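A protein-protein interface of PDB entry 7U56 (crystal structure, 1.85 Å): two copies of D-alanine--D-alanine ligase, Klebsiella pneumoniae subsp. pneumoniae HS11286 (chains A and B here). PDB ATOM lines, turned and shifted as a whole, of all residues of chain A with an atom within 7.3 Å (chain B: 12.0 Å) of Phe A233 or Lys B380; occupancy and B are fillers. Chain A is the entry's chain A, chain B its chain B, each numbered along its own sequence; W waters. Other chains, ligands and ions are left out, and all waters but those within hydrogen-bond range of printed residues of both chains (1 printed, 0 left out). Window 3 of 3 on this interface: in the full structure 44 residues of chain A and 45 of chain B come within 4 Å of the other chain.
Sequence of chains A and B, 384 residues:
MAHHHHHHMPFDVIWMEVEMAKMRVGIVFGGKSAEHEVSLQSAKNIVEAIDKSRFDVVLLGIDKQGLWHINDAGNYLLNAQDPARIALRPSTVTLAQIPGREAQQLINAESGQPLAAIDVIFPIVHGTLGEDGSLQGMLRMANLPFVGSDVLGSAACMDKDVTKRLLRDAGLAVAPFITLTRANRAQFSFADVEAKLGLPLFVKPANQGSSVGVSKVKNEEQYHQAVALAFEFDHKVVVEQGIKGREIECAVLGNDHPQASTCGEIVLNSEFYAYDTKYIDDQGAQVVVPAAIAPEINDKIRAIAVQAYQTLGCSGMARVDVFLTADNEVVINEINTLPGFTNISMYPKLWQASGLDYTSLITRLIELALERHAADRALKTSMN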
ATOM      1  N   THR A 128     -18.357  -1.950 -26.871  1.00  0.00           N
ATOM      2  CA  THR A 128     -17.411  -3.051 -26.760  1.00  0.00           C
ATOM      3  C   THR A 128     -16.673  -3.267 -28.080  1.00  0.00           C
ATOM      4  O   THR A 128     -17.250  -3.135 -29.167  1.00  0.00           O
ATOM      5  CB  THR A 128     -18.144  -4.330 -26.360  1.00  0.00           C
ATOM      6  OG1 THR A 128     -19.249  -3.997 -25.507  1.00  0.00           O
ATOM      7  CG2 THR A 128     -17.204  -5.271 -25.616  1.00  0.00           C
ATOM      8  N   PRO A 205     -22.931  -1.688 -14.595  1.00  0.00           N
ATOM      9  CA  PRO A 205     -21.845  -2.573 -15.022  1.00  0.00           C
ATOM     10  C   PRO A 205     -20.561  -1.774 -15.129  1.00  0.00           C
ATOM     11  O   PRO A 205     -20.574  -0.583 -15.463  1.00  0.00           O
ATOM     12  CB  PRO A 205     -22.310  -3.086 -16.391  1.00  0.00           C
ATOM     13  CG  PRO A 205     -23.287  -2.057 -16.871  1.00  0.00           C
ATOM     14  CD  PRO A 205     -23.930  -1.451 -15.649  1.00  0.00           C
ATOM     15  N   ALA A 206     -19.452  -2.428 -14.786  1.00  0.00           N
ATOM     16  CA  ALA A 206     -18.155  -1.757 -14.840  1.00  0.00           C
ATOM     17  C   ALA A 206     -17.808  -1.341 -16.266  1.00  0.00           C
ATOM     18  O   ALA A 206     -17.252  -0.258 -16.492  1.00  0.00           O
ATOM     19  CB  ALA A 206     -17.071  -2.670 -14.265  1.00  0.00           C
ATOM     20  N   ASN A 207     -18.134  -2.191 -17.237  1.00  0.00           N
ATOM     21  CA  ASN A 207     -17.792  -2.008 -18.641  1.00  0.00           C
ATOM     22  C   ASN A 207     -19.093  -1.996 -19.423  1.00  0.00           C
ATOM     23  O   ASN A 207     -19.728  -3.046 -19.572  1.00  0.00           O
ATOM     24  CB  ASN A 207     -16.900  -3.143 -19.153  1.00  0.00           C
ATOM     25  CG  ASN A 207     -15.502  -3.092 -18.588  1.00  0.00           C
ATOM     26  OD1 ASN A 207     -14.634  -2.405 -19.129  1.00  0.00           O
ATOM     27  ND2 ASN A 207     -15.272  -3.814 -17.499  1.00  0.00           N
ATOM     28  N   GLN A 208     -19.501  -0.826 -19.902  1.00  0.00           N
ATOM     29  CA  GLN A 208     -20.601  -0.773 -20.873  1.00  0.00           C
ATOM     30  C   GLN A 208     -20.665   0.558 -21.631  1.00  0.00           C
ATOM     31  O   GLN A 208     -20.066   1.551 -21.222  1.00  0.00           O
ATOM     32  CB  GLN A 208     -21.939  -1.043 -20.181  1.00  0.00           C
ATOM     33  CG  GLN A 208     -23.091  -1.299 -21.144  1.00  0.00           C
ATOM     34  CD  GLN A 208     -22.886  -2.542 -21.995  1.00  0.00           C
ATOM     35  OE1 GLN A 208     -23.446  -2.656 -23.083  1.00  0.00           O
ATOM     36  NE2 GLN A 208     -22.085  -3.484 -21.497  1.00  0.00           N
ATOM     37  N   VAL A 212     -26.217   1.514 -20.549  1.00  0.00           N
ATOM     38  CA  VAL A 212     -27.007   0.311 -20.346  1.00  0.00           C
ATOM     39  C   VAL A 212     -26.740  -0.265 -18.961  1.00  0.00           C
ATOM     40  O   VAL A 212     -25.599  -0.271 -18.478  1.00  0.00           O
ATOM     41  CB  VAL A 212     -26.678  -0.706 -21.449  1.00  0.00           C
ATOM     42  CG1 VAL A 212     -27.415  -1.963 -21.216  1.00  0.00           C
ATOM     43  CG2 VAL A 212     -27.039  -0.129 -22.812  1.00  0.00           C
ATOM     44  N   GLY A 213     -27.797  -0.760 -18.311  1.00  0.00           N
ATOM     45  CA  GLY A 213     -27.661  -1.446 -17.036  1.00  0.00           C
ATOM     46  C   GLY A 213     -27.499  -0.557 -15.815  1.00  0.00           C
ATOM     47  O   GLY A 213     -27.210  -1.085 -14.729  1.00  0.00           O
ATOM     48  N   VAL A 214     -27.665   0.761 -15.951  1.00  0.00           N
ATOM     49  CA  VAL A 214     -27.498   1.699 -14.838  1.00  0.00           C
ATOM     50  C   VAL A 214     -28.848   1.913 -14.168  1.00  0.00           C
ATOM     51  O   VAL A 214     -29.801   2.350 -14.817  1.00  0.00           O
ATOM     52  CB  VAL A 214     -26.930   3.044 -15.312  1.00  0.00           C
ATOM     53  CG1 VAL A 214     -26.844   4.025 -14.136  1.00  0.00           C
ATOM     54  CG2 VAL A 214     -25.566   2.869 -16.004  1.00  0.00           C
ATOM     55  N   VAL A 227     -28.652  -5.161  -9.290  1.00  0.00           N
ATOM     56  CA  VAL A 227     -27.403  -5.925  -9.308  1.00  0.00           C
ATOM     57  C   VAL A 227     -27.527  -7.098 -10.276  1.00  0.00           C
ATOM     58  O   VAL A 227     -26.643  -7.346 -11.109  1.00  0.00           O
ATOM     59  CB  VAL A 227     -27.049  -6.392  -7.881  1.00  0.00           C
ATOM     60  CG1 VAL A 227     -25.886  -7.402  -7.903  1.00  0.00           C
ATOM     61  CG2 VAL A 227     -26.703  -5.180  -6.999  1.00  0.00           C
ATOM     62  N   ALA A 228     -28.643  -7.819 -10.197  1.00  0.00           N
ATOM     63  CA  ALA A 228     -28.863  -8.933 -11.116  1.00  0.00           C
ATOM     64  C   ALA A 228     -28.838  -8.443 -12.561  1.00  0.00           C
ATOM     65  O   ALA A 228     -28.161  -9.033 -13.418  1.00  0.00           O
ATOM     66  CB  ALA A 228     -30.185  -9.631 -10.775  1.00  0.00           C
ATOM     67  N   LEU A 229     -29.504  -7.311 -12.825  1.00  0.00           N
ATOM     68  CA  LEU A 229     -29.508  -6.722 -14.164  1.00  0.00           C
ATOM     69  C   LEU A 229     -28.101  -6.395 -14.638  1.00  0.00           C
ATOM     70  O   LEU A 229     -27.727  -6.722 -15.768  1.00  0.00           O
ATOM     71  CB  LEU A 229     -30.373  -5.455 -14.171  1.00  0.00           C
ATOM     72  CG  LEU A 229     -30.414  -4.773 -15.541  1.00  0.00           C
ATOM     73  CD1 LEU A 229     -31.144  -5.701 -16.540  1.00  0.00           C
ATOM     74  CD2 LEU A 229     -31.070  -3.387 -15.433  1.00  0.00           C
ATOM     75  N   ALA A 230     -27.309  -5.712 -13.801  1.00  0.00           N
ATOM     76  CA  ALA A 230     -25.971  -5.316 -14.230  1.00  0.00           C
ATOM     77  C   ALA A 230     -25.093  -6.529 -14.523  1.00  0.00           C
ATOM     78  O   ALA A 230     -24.242  -6.479 -15.427  1.00  0.00           O
ATOM     79  CB  ALA A 230     -25.320  -4.419 -13.176  1.00  0.00           C
ATOM     80  N   PHE A 231     -25.282  -7.625 -13.783  1.00  0.00           N
ATOM     81  CA  PHE A 231     -24.513  -8.829 -14.057  1.00  0.00           C
ATOM     82  C   PHE A 231     -24.927  -9.521 -15.343  1.00  0.00           C
ATOM     83  O   PHE A 231     -24.260 -10.481 -15.746  1.00  0.00           O
ATOM     84  CB  PHE A 231     -24.603  -9.803 -12.889  1.00  0.00           C
ATOM     85  CG  PHE A 231     -23.562  -9.552 -11.835  1.00  0.00           C
ATOM     86  CD1 PHE A 231     -22.221  -9.653 -12.145  1.00  0.00           C
ATOM     87  CD2 PHE A 231     -23.926  -9.195 -10.555  1.00  0.00           C
ATOM     88  CE1 PHE A 231     -21.247  -9.425 -11.192  1.00  0.00           C
ATOM     89  CE2 PHE A 231     -22.962  -8.972  -9.575  1.00  0.00           C
ATOM     90  CZ  PHE A 231     -21.612  -9.092  -9.900  1.00  0.00           C
ATOM     91  N   GLU A 232     -26.003  -9.070 -15.998  1.00  0.00           N
ATOM     92  CA  GLU A 232     -26.293  -9.556 -17.343  1.00  0.00           C
ATOM     93  C   GLU A 232     -25.450  -8.862 -18.396  1.00  0.00           C
ATOM     94  O   GLU A 232     -25.349  -9.354 -19.521  1.00  0.00           O
ATOM     95  CB  GLU A 232     -27.776  -9.375 -17.674  1.00  0.00           C
ATOM     96  CG  GLU A 232     -28.649 -10.200 -16.767  1.00  0.00           C
ATOM     97  CD  GLU A 232     -30.054 -10.346 -17.279  1.00  0.00           C
ATOM     98  OE1 GLU A 232     -30.783  -9.331 -17.303  1.00  0.00           O
ATOM     99  OE2 GLU A 232     -30.424 -11.477 -17.669  1.00  0.00           O
ATOM    100  N   PHE A 233     -24.837  -7.736 -18.063  1.00  0.00           N
ATOM    101  CA  PHE A 233     -24.052  -6.995 -19.035  1.00  0.00           C
ATOM    102  C   PHE A 233     -22.557  -7.063 -18.812  1.00  0.00           C
ATOM    103  O   PHE A 233     -21.809  -6.820 -19.755  1.00  0.00           O
ATOM    104  CB  PHE A 233     -24.482  -5.526 -19.047  1.00  0.00           C
ATOM    105  CG  PHE A 233     -25.887  -5.333 -19.501  1.00  0.00           C
ATOM    106  CD1 PHE A 233     -26.206  -5.390 -20.853  1.00  0.00           C
ATOM    107  CD2 PHE A 233     -26.906  -5.115 -18.582  1.00  0.00           C
ATOM    108  CE1 PHE A 233     -27.512  -5.233 -21.284  1.00  0.00           C
ATOM    109  CE2 PHE A 233     -28.216  -4.946 -19.010  1.00  0.00           C
ATOM    110  CZ  PHE A 233     -28.517  -5.012 -20.364  1.00  0.00           C
ATOM    111  N   ASP A 234     -22.097  -7.352 -17.599  1.00  0.00           N
ATOM    112  CA  ASP A 234     -20.662  -7.418 -17.347  1.00  0.00           C
ATOM    113  C   ASP A 234     -20.459  -8.368 -16.177  1.00  0.00           C
ATOM    114  O   ASP A 234     -21.411  -8.719 -15.469  1.00  0.00           O
ATOM    115  CB  ASP A 234     -20.053  -6.031 -17.034  1.00  0.00           C
ATOM    116  CG  ASP A 234     -18.516  -6.038 -17.007  1.00  0.00           C
ATOM    117  OD1 ASP A 234     -17.884  -7.016 -17.475  1.00  0.00           O
ATOM    118  OD2 ASP A 234     -17.926  -5.057 -16.508  1.00  0.00           O
ATOM    119  N   HIS A 235     -19.214  -8.802 -15.999  1.00  0.00           N
ATOM    120  CA  HIS A 235     -18.869  -9.672 -14.880  1.00  0.00           C
ATOM    121  C   HIS A 235     -18.487  -8.885 -13.647  1.00  0.00           C
ATOM    122  O   HIS A 235     -18.200  -9.485 -12.612  1.00  0.00           O
ATOM    123  CB  HIS A 235     -17.724 -10.615 -15.265  1.00  0.00           C
ATOM    124  CG  HIS A 235     -18.017 -11.434 -16.475  1.00  0.00           C
ATOM    125  ND1 HIS A 235     -19.170 -12.176 -16.603  1.00  0.00           N
ATOM    126  CD2 HIS A 235     -17.311 -11.630 -17.614  1.00  0.00           C
ATOM    127  CE1 HIS A 235     -19.165 -12.794 -17.772  1.00  0.00           C
ATOM    128  NE2 HIS A 235     -18.044 -12.484 -18.401  1.00  0.00           N
ATOM    129  N   LYS A 236     -18.499  -7.557 -13.733  1.00  0.00           N
ATOM    130  CA  LYS A 236     -18.197  -6.691 -12.607  1.00  0.00           C
ATOM    131  C   LYS A 236     -19.290  -5.638 -12.509  1.00  0.00           C
ATOM    132  O   LYS A 236     -19.737  -5.111 -13.531  1.00  0.00           O
ATOM    133  CB  LYS A 236     -16.841  -5.988 -12.760  1.00  0.00           C
ATOM    134  CG  LYS A 236     -15.630  -6.854 -12.578  1.00  0.00           C
ATOM    135  CD  LYS A 236     -14.389  -6.210 -13.215  1.00  0.00           C
ATOM    136  CE  LYS A 236     -14.046  -4.875 -12.627  1.00  0.00           C
ATOM    137  NZ  LYS A 236     -12.674  -4.410 -13.074  1.00  0.00           N
ATOM    138  N   VAL A 237     -19.695  -5.322 -11.289  1.00  0.00           N
ATOM    139  CA  VAL A 237     -20.787  -4.389 -11.051  1.00  0.00           C
ATOM    140  C   VAL A 237     -20.319  -3.352 -10.042  1.00  0.00           C
ATOM    141  O   VAL A 237     -19.876  -3.696  -8.940  1.00  0.00           O
ATOM    142  CB  VAL A 237     -22.054  -5.099 -10.550  1.00  0.00           C
ATOM    143  CG1 VAL A 237     -23.111  -4.061 -10.134  1.00  0.00           C
ATOM    144  CG2 VAL A 237     -22.593  -6.004 -11.668  1.00  0.00           C
ATOM    145  N   GLU B 102     -17.130 -13.905 -37.182  1.00  0.00           N
ATOM    146  CA  GLU B 102     -17.161 -14.855 -36.079  1.00  0.00           C
ATOM    147  C   GLU B 102     -16.870 -16.273 -36.529  1.00  0.00           C
ATOM    148  O   GLU B 102     -16.714 -17.163 -35.685  1.00  0.00           O
ATOM    149  CB  GLU B 102     -18.526 -14.794 -35.390  1.00  0.00           C
ATOM    150  CG  GLU B 102     -18.837 -13.378 -34.967  1.00  0.00           C
ATOM    151  CD  GLU B 102     -19.805 -13.306 -33.830  1.00  0.00           C
ATOM    152  OE1 GLU B 102     -20.896 -13.908 -33.941  1.00  0.00           O
ATOM    153  OE2 GLU B 102     -19.462 -12.649 -32.825  1.00  0.00           O
ATOM    154  N   ARG B 140      -9.805 -10.974 -29.699  1.00  0.00           N
ATOM    155  CA  ARG B 140     -11.160 -10.550 -29.373  1.00  0.00           C
ATOM    156  C   ARG B 140     -11.929 -10.097 -30.609  1.00  0.00           C
ATOM    157  O   ARG B 140     -13.115 -10.421 -30.761  1.00  0.00           O
ATOM    158  CB  ARG B 140     -11.113  -9.412 -28.358  1.00  0.00           C
ATOM    159  CG  ARG B 140     -11.077  -9.874 -26.952  1.00  0.00           C
ATOM    160  CD  ARG B 140     -11.181  -8.675 -26.059  1.00  0.00           C
ATOM    161  NE  ARG B 140     -12.369  -7.868 -26.299  1.00  0.00           N
ATOM    162  CZ  ARG B 140     -13.471  -7.928 -25.569  1.00  0.00           C
ATOM    163  NH1 ARG B 140     -13.608  -8.822 -24.607  1.00  0.00           N
ATOM    164  NH2 ARG B 140     -14.454  -7.062 -25.804  1.00  0.00           N
ATOM    165  N   ASP B 150      -7.019 -11.049 -20.451  1.00  0.00           N
ATOM    166  CA  ASP B 150      -7.731 -10.338 -21.512  1.00  0.00           C
ATOM    167  C   ASP B 150      -6.991  -9.029 -21.814  1.00  0.00           C
ATOM    168  O   ASP B 150      -5.864  -8.811 -21.355  1.00  0.00           O
ATOM    169  CB  ASP B 150      -9.187 -10.124 -21.108  1.00  0.00           C
ATOM    170  CG  ASP B 150     -10.147 -10.083 -22.297  1.00  0.00           C
ATOM    171  OD1 ASP B 150      -9.720  -9.928 -23.457  1.00  0.00           O
ATOM    172  OD2 ASP B 150     -11.361 -10.201 -22.048  1.00  0.00           O
ATOM    173  N   ARG B 372     -14.013 -18.847 -19.704  1.00  0.00           N
ATOM    174  CA  ARG B 372     -14.144 -17.396 -19.759  1.00  0.00           C
ATOM    175  C   ARG B 372     -14.914 -16.952 -21.002  1.00  0.00           C
ATOM    176  O   ARG B 372     -15.766 -16.060 -20.927  1.00  0.00           O
ATOM    177  CB  ARG B 372     -12.763 -16.737 -19.717  1.00  0.00           C
ATOM    178  CG  ARG B 372     -12.849 -15.200 -19.642  1.00  0.00           C
ATOM    179  CD  ARG B 372     -11.490 -14.571 -19.426  1.00  0.00           C
ATOM    180  NE  ARG B 372     -10.636 -14.723 -20.600  1.00  0.00           N
ATOM    181  CZ  ARG B 372     -10.606 -13.874 -21.616  1.00  0.00           C
ATOM    182  NH1 ARG B 372     -11.445 -12.850 -21.686  1.00  0.00           N
ATOM    183  NH2 ARG B 372      -9.729 -14.067 -22.597  1.00  0.00           N
ATOM    184  N   HIS B 373     -14.630 -17.561 -22.156  1.00  0.00           N
ATOM    185  CA  HIS B 373     -15.399 -17.271 -23.369  1.00  0.00           C
ATOM    186  C   HIS B 373     -16.877 -17.583 -23.190  1.00  0.00           C
ATOM    187  O   HIS B 373     -17.741 -16.802 -23.616  1.00  0.00           O
ATOM    188  CB  HIS B 373     -14.855 -18.077 -24.546  1.00  0.00           C
ATOM    189  CG  HIS B 373     -15.350 -17.605 -25.878  1.00  0.00           C
ATOM    190  ND1 HIS B 373     -16.261 -18.315 -26.630  1.00  0.00           N
ATOM    191  CD2 HIS B 373     -15.057 -16.493 -26.591  1.00  0.00           C
ATOM    192  CE1 HIS B 373     -16.494 -17.672 -27.758  1.00  0.00           C
ATOM    193  NE2 HIS B 373     -15.787 -16.559 -27.756  1.00  0.00           N
ATOM    194  N   ALA B 374     -17.189 -18.737 -22.588  1.00  0.00           N
ATOM    195  CA  ALA B 374     -18.585 -19.120 -22.375  1.00  0.00           C
ATOM    196  C   ALA B 374     -19.297 -18.151 -21.442  1.00  0.00           C
ATOM    197  O   ALA B 374     -20.495 -17.869 -21.620  1.00  0.00           O
ATOM    198  CB  ALA B 374     -18.662 -20.528 -21.798  1.00  0.00           C
ATOM    199  N   ALA B 375     -18.588 -17.652 -20.421  1.00  0.00           N
ATOM    200  CA  ALA B 375     -19.163 -16.618 -19.559  1.00  0.00           C
ATOM    201  C   ALA B 375     -19.428 -15.340 -20.352  1.00  0.00           C
ATOM    202  O   ALA B 375     -20.501 -14.731 -20.237  1.00  0.00           O
ATOM    203  CB  ALA B 375     -18.232 -16.338 -18.371  1.00  0.00           C
ATOM    204  N   ASP B 376     -18.445 -14.901 -21.138  1.00  0.00           N
ATOM    205  CA  ASP B 376     -18.615 -13.684 -21.923  1.00  0.00           C
ATOM    206  C   ASP B 376     -19.741 -13.839 -22.922  1.00  0.00           C
ATOM    207  O   ASP B 376     -20.545 -12.917 -23.116  1.00  0.00           O
ATOM    208  CB  ASP B 376     -17.325 -13.331 -22.658  1.00  0.00           C
ATOM    209  CG  ASP B 376     -16.183 -12.971 -21.711  1.00  0.00           C
ATOM    210  OD1 ASP B 376     -16.453 -12.613 -20.556  1.00  0.00           O
ATOM    211  OD2 ASP B 376     -15.011 -13.055 -22.123  1.00  0.00           O
ATOM    212  N   ARG B 377     -19.824 -15.008 -23.562  1.00  0.00           N
ATOM    213  CA  ARG B 377     -20.825 -15.207 -24.597  1.00  0.00           C
ATOM    214  C   ARG B 377     -22.241 -15.188 -24.025  1.00  0.00           C
ATOM    215  O   ARG B 377     -23.185 -14.815 -24.729  1.00  0.00           O
ATOM    216  CB  ARG B 377     -20.528 -16.518 -25.337  1.00  0.00           C
ATOM    217  N   ALA B 378     -22.411 -15.553 -22.749  1.00  0.00           N
ATOM    218  CA  ALA B 378     -23.730 -15.550 -22.123  1.00  0.00           C
ATOM    219  C   ALA B 378     -24.224 -14.159 -21.741  1.00  0.00           C
ATOM    220  O   ALA B 378     -25.406 -14.010 -21.416  1.00  0.00           O
ATOM    221  CB  ALA B 378     -23.730 -16.442 -20.878  1.00  0.00           C
ATOM    222  N   LEU B 379     -23.367 -13.148 -21.769  1.00  0.00           N
ATOM    223  CA  LEU B 379     -23.783 -11.796 -21.428  1.00  0.00           C
ATOM    224  C   LEU B 379     -24.765 -11.262 -22.461  1.00  0.00           C
ATOM    225  O   LEU B 379     -24.725 -11.632 -23.639  1.00  0.00           O
ATOM    226  CB  LEU B 379     -22.572 -10.868 -21.352  1.00  0.00           C
ATOM    227  CG  LEU B 379     -21.535 -11.151 -20.268  1.00  0.00           C
ATOM    228  CD1 LEU B 379     -20.340 -10.226 -20.405  1.00  0.00           C
ATOM    229  CD2 LEU B 379     -22.156 -11.050 -18.889  1.00  0.00           C
ATOM    230  N   LYS B 380     -25.677 -10.413 -21.998  1.00  0.00           N
ATOM    231  CA  LYS B 380     -26.510  -9.654 -22.919  1.00  0.00           C
ATOM    232  C   LYS B 380     -25.667  -8.590 -23.605  1.00  0.00           C
ATOM    233  O   LYS B 380     -24.714  -8.050 -23.032  1.00  0.00           O
ATOM    234  CB  LYS B 380     -27.678  -8.994 -22.181  1.00  0.00           C
ATOM    235  CG  LYS B 380     -28.670  -9.961 -21.601  1.00  0.00           C
ATOM    236  CD  LYS B 380     -29.690  -9.251 -20.727  1.00  0.00           C
ATOM    237  CE  LYS B 380     -30.031  -7.880 -21.269  1.00  0.00           C
ATOM    238  NZ  LYS B 380     -30.920  -7.928 -22.471  1.00  0.00           N
ATOM    239  N   THR B 381     -26.024  -8.287 -24.846  1.00  0.00           N
ATOM    240  CA  THR B 381     -25.316  -7.277 -25.622  1.00  0.00           C
ATOM    241  C   THR B 381     -26.235  -6.110 -25.990  1.00  0.00           C
ATOM    242  O   THR B 381     -25.943  -4.955 -25.670  1.00  0.00           O
ATOM    243  CB  THR B 381     -24.726  -7.883 -26.901  1.00  0.00           C
ATOM    244  OG1 THR B 381     -25.739  -8.644 -27.567  1.00  0.00           O
ATOM    245  CG2 THR B 381     -23.567  -8.790 -26.563  1.00  0.00           C
HETATM  246  O   HOH W   1     -22.473  -6.659 -22.285  1.00  0.00           O
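Phe A233 touches two residues of chain B. Lys B380 touches just these residues of chain A: Glu A232 and Phe A233. Pro A205 touches none of the printed residues of chain B. No residue of chain B comes within 4 Å of Val A212. No residue of chain B comes within 4 Å of Gly A213. No residue of chain B comes within 4 Å of Ala A230. Of the printed residues of chain B, Asp A234 touches Leu B379 (3.9 Å). Printed residues of chain B within 4 Å of Phe A231: Leu B379. Of the printed residues of chain A, Asp B376 touches His A235 (2.7 Å). Of the printed residues of chain B, His A235 touches Ala B375 (3.4 Å), Asp B376 (2.7 Å) and Leu B379 (3.6 Å). Of the printed residues of chain A, Leu B379 touches Phe A231, Glu A232, Phe A233, Asp A234 and His A235. Printed residues of chain A within 4 Å of Arg B140: Thr A128 (3.3 Å). Ala B374 touches none of the printed residues of chain A. Arg B372 touches none of the printed residues of chain A. The nearest residue of chain B that does not touch Phe A233 is Thr B381 (4.7 Å). The nearest residue of chain A that does not touch Lys B380 is Leu A229 (5.3 Å). The nearest printed residue of chain B that does not touch Phe A231 is Lys B380 (6.4 Å).
Of the 13 printed residues of chain B, 5 touch a printed residue of chain A. Of the 19 printed residues of chain A, 6 touch a printed residue of chain B. Printed residues of chain A that touch a printed residue of chain B: Thr A128, Phe A231, Glu A232, Phe A233, Asp A234 and His A235. Among the printed residues, 10 pairs touch across the chains. Among the printed residues, no Asp or Glu carboxylate lies within 4 Å of a Lys or Arg side-chain nitrogen of the other chain.
OD2 of Asp A234 sits close to N of Ala A206 (3.5 Å). The backbone NH (N) of Asn A207 is in hydrogen-bond range of the side-chain carboxylate (OD2) of Asp A234, at 3.0 Å. The side-chain carboxylate (OD2) of Asp B150 lies within salt-bridge range of the guanidinium group (NH1) of Arg B140, 3.7 Å away. OD2 of Asp B376 is in salt-bridge range of NH1 of Arg B372 (3.6 Å).
Water W1 lies within hydrogen-bond range of the backbone carbonyl oxygen of Phe A233 (2.6 Å), the backbone carbonyl oxygen of Lys B380 (2.7 Å) and the side-chain amide nitrogen of Gln A208 (3.3 Å).
The backbone NH (N) of Lys B380 lies within hydrogen-bond range of the backbone carbonyl oxygen (O) of Glu A232 (2.7 Å). The side-chain carboxylate (OD1) of Asp B376 is in hydrogen-bond range of a ring nitrogen (NE2) of His A235, at 2.7 Å.
Arg B140 touches Thr A128 (NH2 to CG2, 3.3 Å). Leu B379 touches Phe A231 (CD2 to O, 3.8 Å). O of Glu A232 touches CA of Leu B379, at 3.5 Å. Phe A233 touches Leu B379. Phe A233 touches Lys B380 (CZ to CE, 3.4 Å). Asp A234 touches Leu B379 (N to CD2, 3.9 Å). His A235 touches Ala B375. His A235 touches Leu B379 (CE1 to CD2, 3.6 Å).
No position is printed for both chains.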
